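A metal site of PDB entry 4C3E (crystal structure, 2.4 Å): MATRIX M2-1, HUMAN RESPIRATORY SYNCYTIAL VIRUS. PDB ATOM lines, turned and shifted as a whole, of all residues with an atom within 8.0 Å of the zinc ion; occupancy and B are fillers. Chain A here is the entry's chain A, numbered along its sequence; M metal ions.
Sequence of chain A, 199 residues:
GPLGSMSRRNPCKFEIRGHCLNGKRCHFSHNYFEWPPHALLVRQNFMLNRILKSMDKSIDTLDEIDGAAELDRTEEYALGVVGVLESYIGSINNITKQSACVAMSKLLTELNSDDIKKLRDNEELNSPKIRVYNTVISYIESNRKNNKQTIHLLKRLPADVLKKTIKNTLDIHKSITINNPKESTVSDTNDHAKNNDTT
Four residues have an atom within 4 Å of the zinc ion: Cys 12, Cys 20, Cys 26 and His 30.
The nearest printed residue that does not touch the zinc ion is Phe 28 (4.8 Å).
The backbone carbonyl oxygen (O) of Phe 28 lies within hydrogen-bond range of a ring nitrogen (ND1) of His 30, at 3.0 Å.
N of Asn 22 lies close to SG of Cys 20 (3.6 Å).
The side-chain carboxylate (OE1) of Glu 15 is in hydrogen-bond range of the backbone NH (N) of Cys 20 (2.9 Å).
The backbone NH (N) of Phe 28 sits close to the side-chain sulfur (SG) of Cys 26, at 3.5 Å.
SG of Cys 12 lies close to N of Phe 14, 3.3 Å away.
N of Glu 15 lies close to SG of Cys 12 (3.6 Å).
The backbone carbonyl oxygen (O) of Ser 29 lies within hydrogen-bond range of the backbone NH (N) of Cys 12.
NE2 of His 30 is bound to the zinc ion (2.0 Å).
SG of Cys 20 is bound to the zinc ion (2.2 Å).
SG of Cys 26 binds the zinc ion (2.3 Å).
The side-chain sulfur (SG) of Cys 12 binds the zinc ion (2.3 Å).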
ATOM      1  N   ASN A  10      16.097   9.819  20.571  1.00  0.00           N
ATOM      2  CA  ASN A  10      16.303  10.224  19.201  1.00  0.00           C
ATOM      3  C   ASN A  10      17.780  10.376  18.925  1.00  0.00           C
ATOM      4  O   ASN A  10      18.558  10.641  19.833  1.00  0.00           O
ATOM      5  CB  ASN A  10      15.615  11.551  18.942  1.00  0.00           C
ATOM      6  CG  ASN A  10      14.109  11.416  18.903  1.00  0.00           C
ATOM      7  OD1 ASN A  10      13.556  10.489  18.320  1.00  0.00           O
ATOM      8  ND2 ASN A  10      13.431  12.371  19.495  1.00  0.00           N
ATOM      9  N   PRO A  11      18.169  10.194  17.671  1.00  0.00           N
ATOM     10  CA  PRO A  11      19.542  10.352  17.303  1.00  0.00           C
ATOM     11  C   PRO A  11      20.031  11.779  17.426  1.00  0.00           C
ATOM     12  O   PRO A  11      19.312  12.713  17.202  1.00  0.00           O
ATOM     13  CB  PRO A  11      19.584   9.940  15.853  1.00  0.00           C
ATOM     14  CG  PRO A  11      18.192   9.873  15.388  1.00  0.00           C
ATOM     15  CD  PRO A  11      17.330   9.691  16.585  1.00  0.00           C
ATOM     16  N   CYS A  12      21.266  11.911  17.838  1.00  0.00           N
ATOM     17  CA  CYS A  12      21.833  13.192  18.039  1.00  0.00           C
ATOM     18  C   CYS A  12      22.149  13.822  16.688  1.00  0.00           C
ATOM     19  O   CYS A  12      22.982  13.325  15.922  1.00  0.00           O
ATOM     20  CB  CYS A  12      23.050  13.053  18.893  1.00  0.00           C
ATOM     21  SG  CYS A  12      24.033  14.522  18.979  1.00  0.00           S
ATOM     22  N   LYS A  13      21.595  15.017  16.501  1.00  0.00           N
ATOM     23  CA  LYS A  13      21.766  15.747  15.291  1.00  0.00           C
ATOM     24  C   LYS A  13      23.194  16.123  15.088  1.00  0.00           C
ATOM     25  O   LYS A  13      23.630  16.289  13.939  1.00  0.00           O
ATOM     26  CB  LYS A  13      20.802  16.968  15.209  1.00  0.00           C
ATOM     27  CG  LYS A  13      19.356  16.488  14.998  1.00  0.00           C
ATOM     28  CD  LYS A  13      18.220  17.531  15.117  1.00  0.00           C
ATOM     29  CE  LYS A  13      18.129  18.527  13.937  1.00  0.00           C
ATOM     30  NZ  LYS A  13      18.649  18.048  12.621  1.00  0.00           N
ATOM     31  N   PHE A  14      23.956  16.267  16.139  1.00  0.00           N
ATOM     32  CA  PHE A  14      25.356  16.569  15.892  1.00  0.00           C
ATOM     33  C   PHE A  14      26.104  15.370  15.368  1.00  0.00           C
ATOM     34  O   PHE A  14      27.079  15.503  14.613  1.00  0.00           O
ATOM     35  CB  PHE A  14      26.061  17.071  17.164  1.00  0.00           C
ATOM     36  CG  PHE A  14      25.559  18.414  17.614  1.00  0.00           C
ATOM     37  CD1 PHE A  14      26.121  19.572  17.102  1.00  0.00           C
ATOM     38  CD2 PHE A  14      24.565  18.512  18.539  1.00  0.00           C
ATOM     39  CE1 PHE A  14      25.663  20.816  17.531  1.00  0.00           C
ATOM     40  CE2 PHE A  14      24.090  19.742  18.974  1.00  0.00           C
ATOM     41  CZ  PHE A  14      24.630  20.900  18.450  1.00  0.00           C
ATOM     42  N   GLU A  15      25.705  14.196  15.812  1.00  0.00           N
ATOM     43  CA  GLU A  15      26.372  12.948  15.486  1.00  0.00           C
ATOM     44  C   GLU A  15      25.973  12.642  14.039  1.00  0.00           C
ATOM     45  O   GLU A  15      26.783  12.199  13.281  1.00  0.00           O
ATOM     46  CB  GLU A  15      25.898  11.832  16.430  1.00  0.00           C
ATOM     47  CG  GLU A  15      26.600  10.491  16.300  1.00  0.00           C
ATOM     48  CD  GLU A  15      28.049  10.515  16.708  1.00  0.00           C
ATOM     49  OE1 GLU A  15      28.442  11.440  17.444  1.00  0.00           O
ATOM     50  OE2 GLU A  15      28.822   9.602  16.318  1.00  0.00           O
ATOM     51  N   ILE A  16      24.715  12.908  13.687  1.00  0.00           N
ATOM     52  CA  ILE A  16      24.276  12.750  12.315  1.00  0.00           C
ATOM     53  C   ILE A  16      25.160  13.509  11.340  1.00  0.00           C
ATOM     54  O   ILE A  16      25.365  13.026  10.276  1.00  0.00           O
ATOM     55  CB  ILE A  16      22.833  13.164  12.136  1.00  0.00           C
ATOM     56  CG1 ILE A  16      21.931  12.219  12.889  1.00  0.00           C
ATOM     57  CG2 ILE A  16      22.495  13.096  10.669  1.00  0.00           C
ATOM     58  CD1 ILE A  16      20.482  12.600  12.868  1.00  0.00           C
ATOM     59  N   HIS A  19      30.576  13.976  14.460  1.00  0.00           N
ATOM     60  CA  HIS A  19      30.797  13.563  15.826  1.00  0.00           C
ATOM     61  C   HIS A  19      30.210  14.597  16.778  1.00  0.00           C
ATOM     62  O   HIS A  19      30.637  15.737  16.790  1.00  0.00           O
ATOM     63  CB  HIS A  19      32.307  13.456  16.009  1.00  0.00           C
ATOM     64  CG  HIS A  19      32.938  12.356  15.208  1.00  0.00           C
ATOM     65  ND1 HIS A  19      32.553  11.035  15.345  1.00  0.00           N
ATOM     66  CD2 HIS A  19      33.885  12.382  14.237  1.00  0.00           C
ATOM     67  CE1 HIS A  19      33.242  10.298  14.500  1.00  0.00           C
ATOM     68  NE2 HIS A  19      34.044  11.095  13.814  1.00  0.00           N
ATOM     69  N   CYS A  20      29.303  14.170  17.646  1.00  0.00           N
ATOM     70  CA  CYS A  20      28.842  14.962  18.809  1.00  0.00           C
ATOM     71  C   CYS A  20      29.971  15.319  19.733  1.00  0.00           C
ATOM     72  O   CYS A  20      30.840  14.496  19.973  1.00  0.00           O
ATOM     73  CB  CYS A  20      27.856  14.180  19.651  1.00  0.00           C
ATOM     74  SG  CYS A  20      27.063  15.246  20.884  1.00  0.00           S
ATOM     75  N   LEU A  21      30.077  16.589  20.067  1.00  0.00           N
ATOM     76  CA  LEU A  21      31.281  17.095  20.792  1.00  0.00           C
ATOM     77  C   LEU A  21      30.874  17.538  22.202  1.00  0.00           C
ATOM     78  O   LEU A  21      31.602  18.185  22.881  1.00  0.00           O
ATOM     79  CB  LEU A  21      31.889  18.270  20.064  1.00  0.00           C
ATOM     80  CG  LEU A  21      32.650  18.027  18.753  1.00  0.00           C
ATOM     81  CD1 LEU A  21      33.061  19.402  18.217  1.00  0.00           C
ATOM     82  CD2 LEU A  21      33.887  17.139  18.882  1.00  0.00           C
ATOM     83  N   ASN A  22      29.649  17.200  22.555  1.00  0.00           N
ATOM     84  CA  ASN A  22      29.041  17.624  23.785  1.00  0.00           C
ATOM     85  C   ASN A  22      29.268  16.614  24.940  1.00  0.00           C
ATOM     86  O   ASN A  22      28.587  16.694  25.941  1.00  0.00           O
ATOM     87  CB  ASN A  22      27.512  17.771  23.529  1.00  0.00           C
ATOM     88  CG  ASN A  22      27.137  19.019  22.715  1.00  0.00           C
ATOM     89  OD1 ASN A  22      26.070  19.082  22.017  1.00  0.00           O
ATOM     90  ND2 ASN A  22      28.009  20.015  22.763  1.00  0.00           N
ATOM     91  N   GLY A  23      30.183  15.650  24.794  1.00  0.00           N
ATOM     92  CA  GLY A  23      30.408  14.590  25.818  1.00  0.00           C
ATOM     93  C   GLY A  23      29.150  14.013  26.443  1.00  0.00           C
ATOM     94  O   GLY A  23      28.149  13.878  25.793  1.00  0.00           O
ATOM     95  N   LYS A  24      29.177  13.775  27.772  1.00  0.00           N
ATOM     96  CA  LYS A  24      28.056  13.145  28.489  1.00  0.00           C
ATOM     97  C   LYS A  24      26.882  14.080  28.767  1.00  0.00           C
ATOM     98  O   LYS A  24      25.791  13.648  29.075  1.00  0.00           O
ATOM     99  CB  LYS A  24      28.542  12.562  29.781  1.00  0.00           C
ATOM    100  CG  LYS A  24      29.372  11.306  29.603  1.00  0.00           C
ATOM    101  CD  LYS A  24      29.740  10.677  30.948  1.00  0.00           C
ATOM    102  CE  LYS A  24      28.532  10.116  31.699  1.00  0.00           C
ATOM    103  NZ  LYS A  24      28.897   9.728  33.099  1.00  0.00           N
ATOM    104  N   ARG A  25      27.088  15.362  28.613  1.00  0.00           N
ATOM    105  CA  ARG A  25      25.986  16.317  28.740  1.00  0.00           C
ATOM    106  C   ARG A  25      24.859  16.072  27.710  1.00  0.00           C
ATOM    107  O   ARG A  25      23.700  16.340  27.995  1.00  0.00           O
ATOM    108  CB  ARG A  25      26.506  17.743  28.567  1.00  0.00           C
ATOM    109  CG  ARG A  25      27.706  18.100  29.469  1.00  0.00           C
ATOM    110  CD  ARG A  25      28.870  18.751  28.721  1.00  0.00           C
ATOM    111  NE  ARG A  25      28.737  20.204  28.618  1.00  0.00           N
ATOM    112  CZ  ARG A  25      27.760  20.819  27.944  1.00  0.00           C
ATOM    113  NH1 ARG A  25      26.813  20.128  27.339  1.00  0.00           N
ATOM    114  NH2 ARG A  25      27.727  22.143  27.890  1.00  0.00           N
ATOM    115  N   CYS A  26      25.202  15.495  26.547  1.00  0.00           N
ATOM    116  CA  CYS A  26      24.200  15.273  25.485  1.00  0.00           C
ATOM    117  C   CYS A  26      23.295  14.121  25.816  1.00  0.00           C
ATOM    118  O   CYS A  26      23.727  13.034  26.095  1.00  0.00           O
ATOM    119  CB  CYS A  26      24.855  15.085  24.093  1.00  0.00           C
ATOM    120  SG  CYS A  26      23.651  14.962  22.732  1.00  0.00           S
ATOM    121  N   HIS A  27      22.000  14.377  25.765  1.00  0.00           N
ATOM    122  CA  HIS A  27      20.991  13.401  26.124  1.00  0.00           C
ATOM    123  C   HIS A  27      20.429  12.650  24.912  1.00  0.00           C
ATOM    124  O   HIS A  27      19.561  11.807  25.069  1.00  0.00           O
ATOM    125  CB  HIS A  27      19.856  14.104  26.893  1.00  0.00           C
ATOM    126  CG  HIS A  27      20.295  14.759  28.181  1.00  0.00           C
ATOM    127  ND1 HIS A  27      20.962  14.070  29.171  1.00  0.00           N
ATOM    128  CD2 HIS A  27      20.154  16.031  28.633  1.00  0.00           C
ATOM    129  CE1 HIS A  27      21.222  14.893  30.172  1.00  0.00           C
ATOM    130  NE2 HIS A  27      20.738  16.089  29.864  1.00  0.00           N
ATOM    131  N   PHE A  28      20.912  12.936  23.720  1.00  0.00           N
ATOM    132  CA  PHE A  28      20.435  12.196  22.547  1.00  0.00           C
ATOM    133  C   PHE A  28      21.247  10.911  22.316  1.00  0.00           C
ATOM    134  O   PHE A  28      22.286  10.716  22.919  1.00  0.00           O
ATOM    135  CB  PHE A  28      20.471  13.070  21.292  1.00  0.00           C
ATOM    136  CG  PHE A  28      19.514  14.223  21.307  1.00  0.00           C
ATOM    137  CD1 PHE A  28      19.809  15.369  22.041  1.00  0.00           C
ATOM    138  CD2 PHE A  28      18.312  14.161  20.600  1.00  0.00           C
ATOM    139  CE1 PHE A  28      18.923  16.423  22.091  1.00  0.00           C
ATOM    140  CE2 PHE A  28      17.428  15.239  20.628  1.00  0.00           C
ATOM    141  CZ  PHE A  28      17.738  16.374  21.378  1.00  0.00           C
ATOM    142  N   SER A  29      20.770  10.050  21.429  1.00  0.00           N
ATOM    143  CA  SER A  29      21.450   8.775  21.159  1.00  0.00           C
ATOM    144  C   SER A  29      22.649   8.902  20.265  1.00  0.00           C
ATOM    145  O   SER A  29      22.567   9.510  19.207  1.00  0.00           O
ATOM    146  CB  SER A  29      20.545   7.765  20.480  1.00  0.00           C
ATOM    147  OG  SER A  29      21.377   6.642  20.142  1.00  0.00           O
ATOM    148  N   HIS A  30      23.755   8.344  20.727  1.00  0.00           N
ATOM    149  CA  HIS A  30      24.982   8.263  19.984  1.00  0.00           C
ATOM    150  C   HIS A  30      25.244   6.783  19.671  1.00  0.00           C
ATOM    151  O   HIS A  30      26.329   6.416  19.244  1.00  0.00           O
ATOM    152  CB  HIS A  30      26.156   8.832  20.768  1.00  0.00           C
ATOM    153  CG  HIS A  30      25.905  10.243  21.199  1.00  0.00           C
ATOM    154  ND1 HIS A  30      25.226  10.542  22.353  1.00  0.00           N
ATOM    155  CD2 HIS A  30      26.146  11.432  20.571  1.00  0.00           C
ATOM    156  CE1 HIS A  30      25.066  11.851  22.426  1.00  0.00           C
ATOM    157  NE2 HIS A  30      25.637  12.420  21.369  1.00  0.00           N
ATOM    158  N   TRP A  35      19.466   3.760  16.098  1.00  0.00           N
ATOM    159  CA  TRP A  35      19.029   4.787  15.142  1.00  0.00           C
ATOM    160  C   TRP A  35      18.088   4.248  14.094  1.00  0.00           C
ATOM    161  O   TRP A  35      18.223   3.122  13.641  1.00  0.00           O
ATOM    162  CB  TRP A  35      20.233   5.377  14.433  1.00  0.00           C
ATOM    163  CG  TRP A  35      21.025   6.290  15.276  1.00  0.00           C
ATOM    164  CD1 TRP A  35      21.025   6.380  16.642  1.00  0.00           C
ATOM    165  CD2 TRP A  35      21.936   7.280  14.811  1.00  0.00           C
ATOM    166  NE1 TRP A  35      21.919   7.314  17.038  1.00  0.00           N
ATOM    167  CE2 TRP A  35      22.467   7.907  15.926  1.00  0.00           C
ATOM    168  CE3 TRP A  35      22.309   7.722  13.536  1.00  0.00           C
ATOM    169  CZ2 TRP A  35      23.371   8.963  15.837  1.00  0.00           C
ATOM    170  CZ3 TRP A  35      23.228   8.713  13.444  1.00  0.00           C
ATOM    171  CH2 TRP A  35      23.776   9.329  14.596  1.00  0.00           C
HETATM  172 ZN    ZN M   1      25.081  14.337  21.040  1.00  0.00          ZN
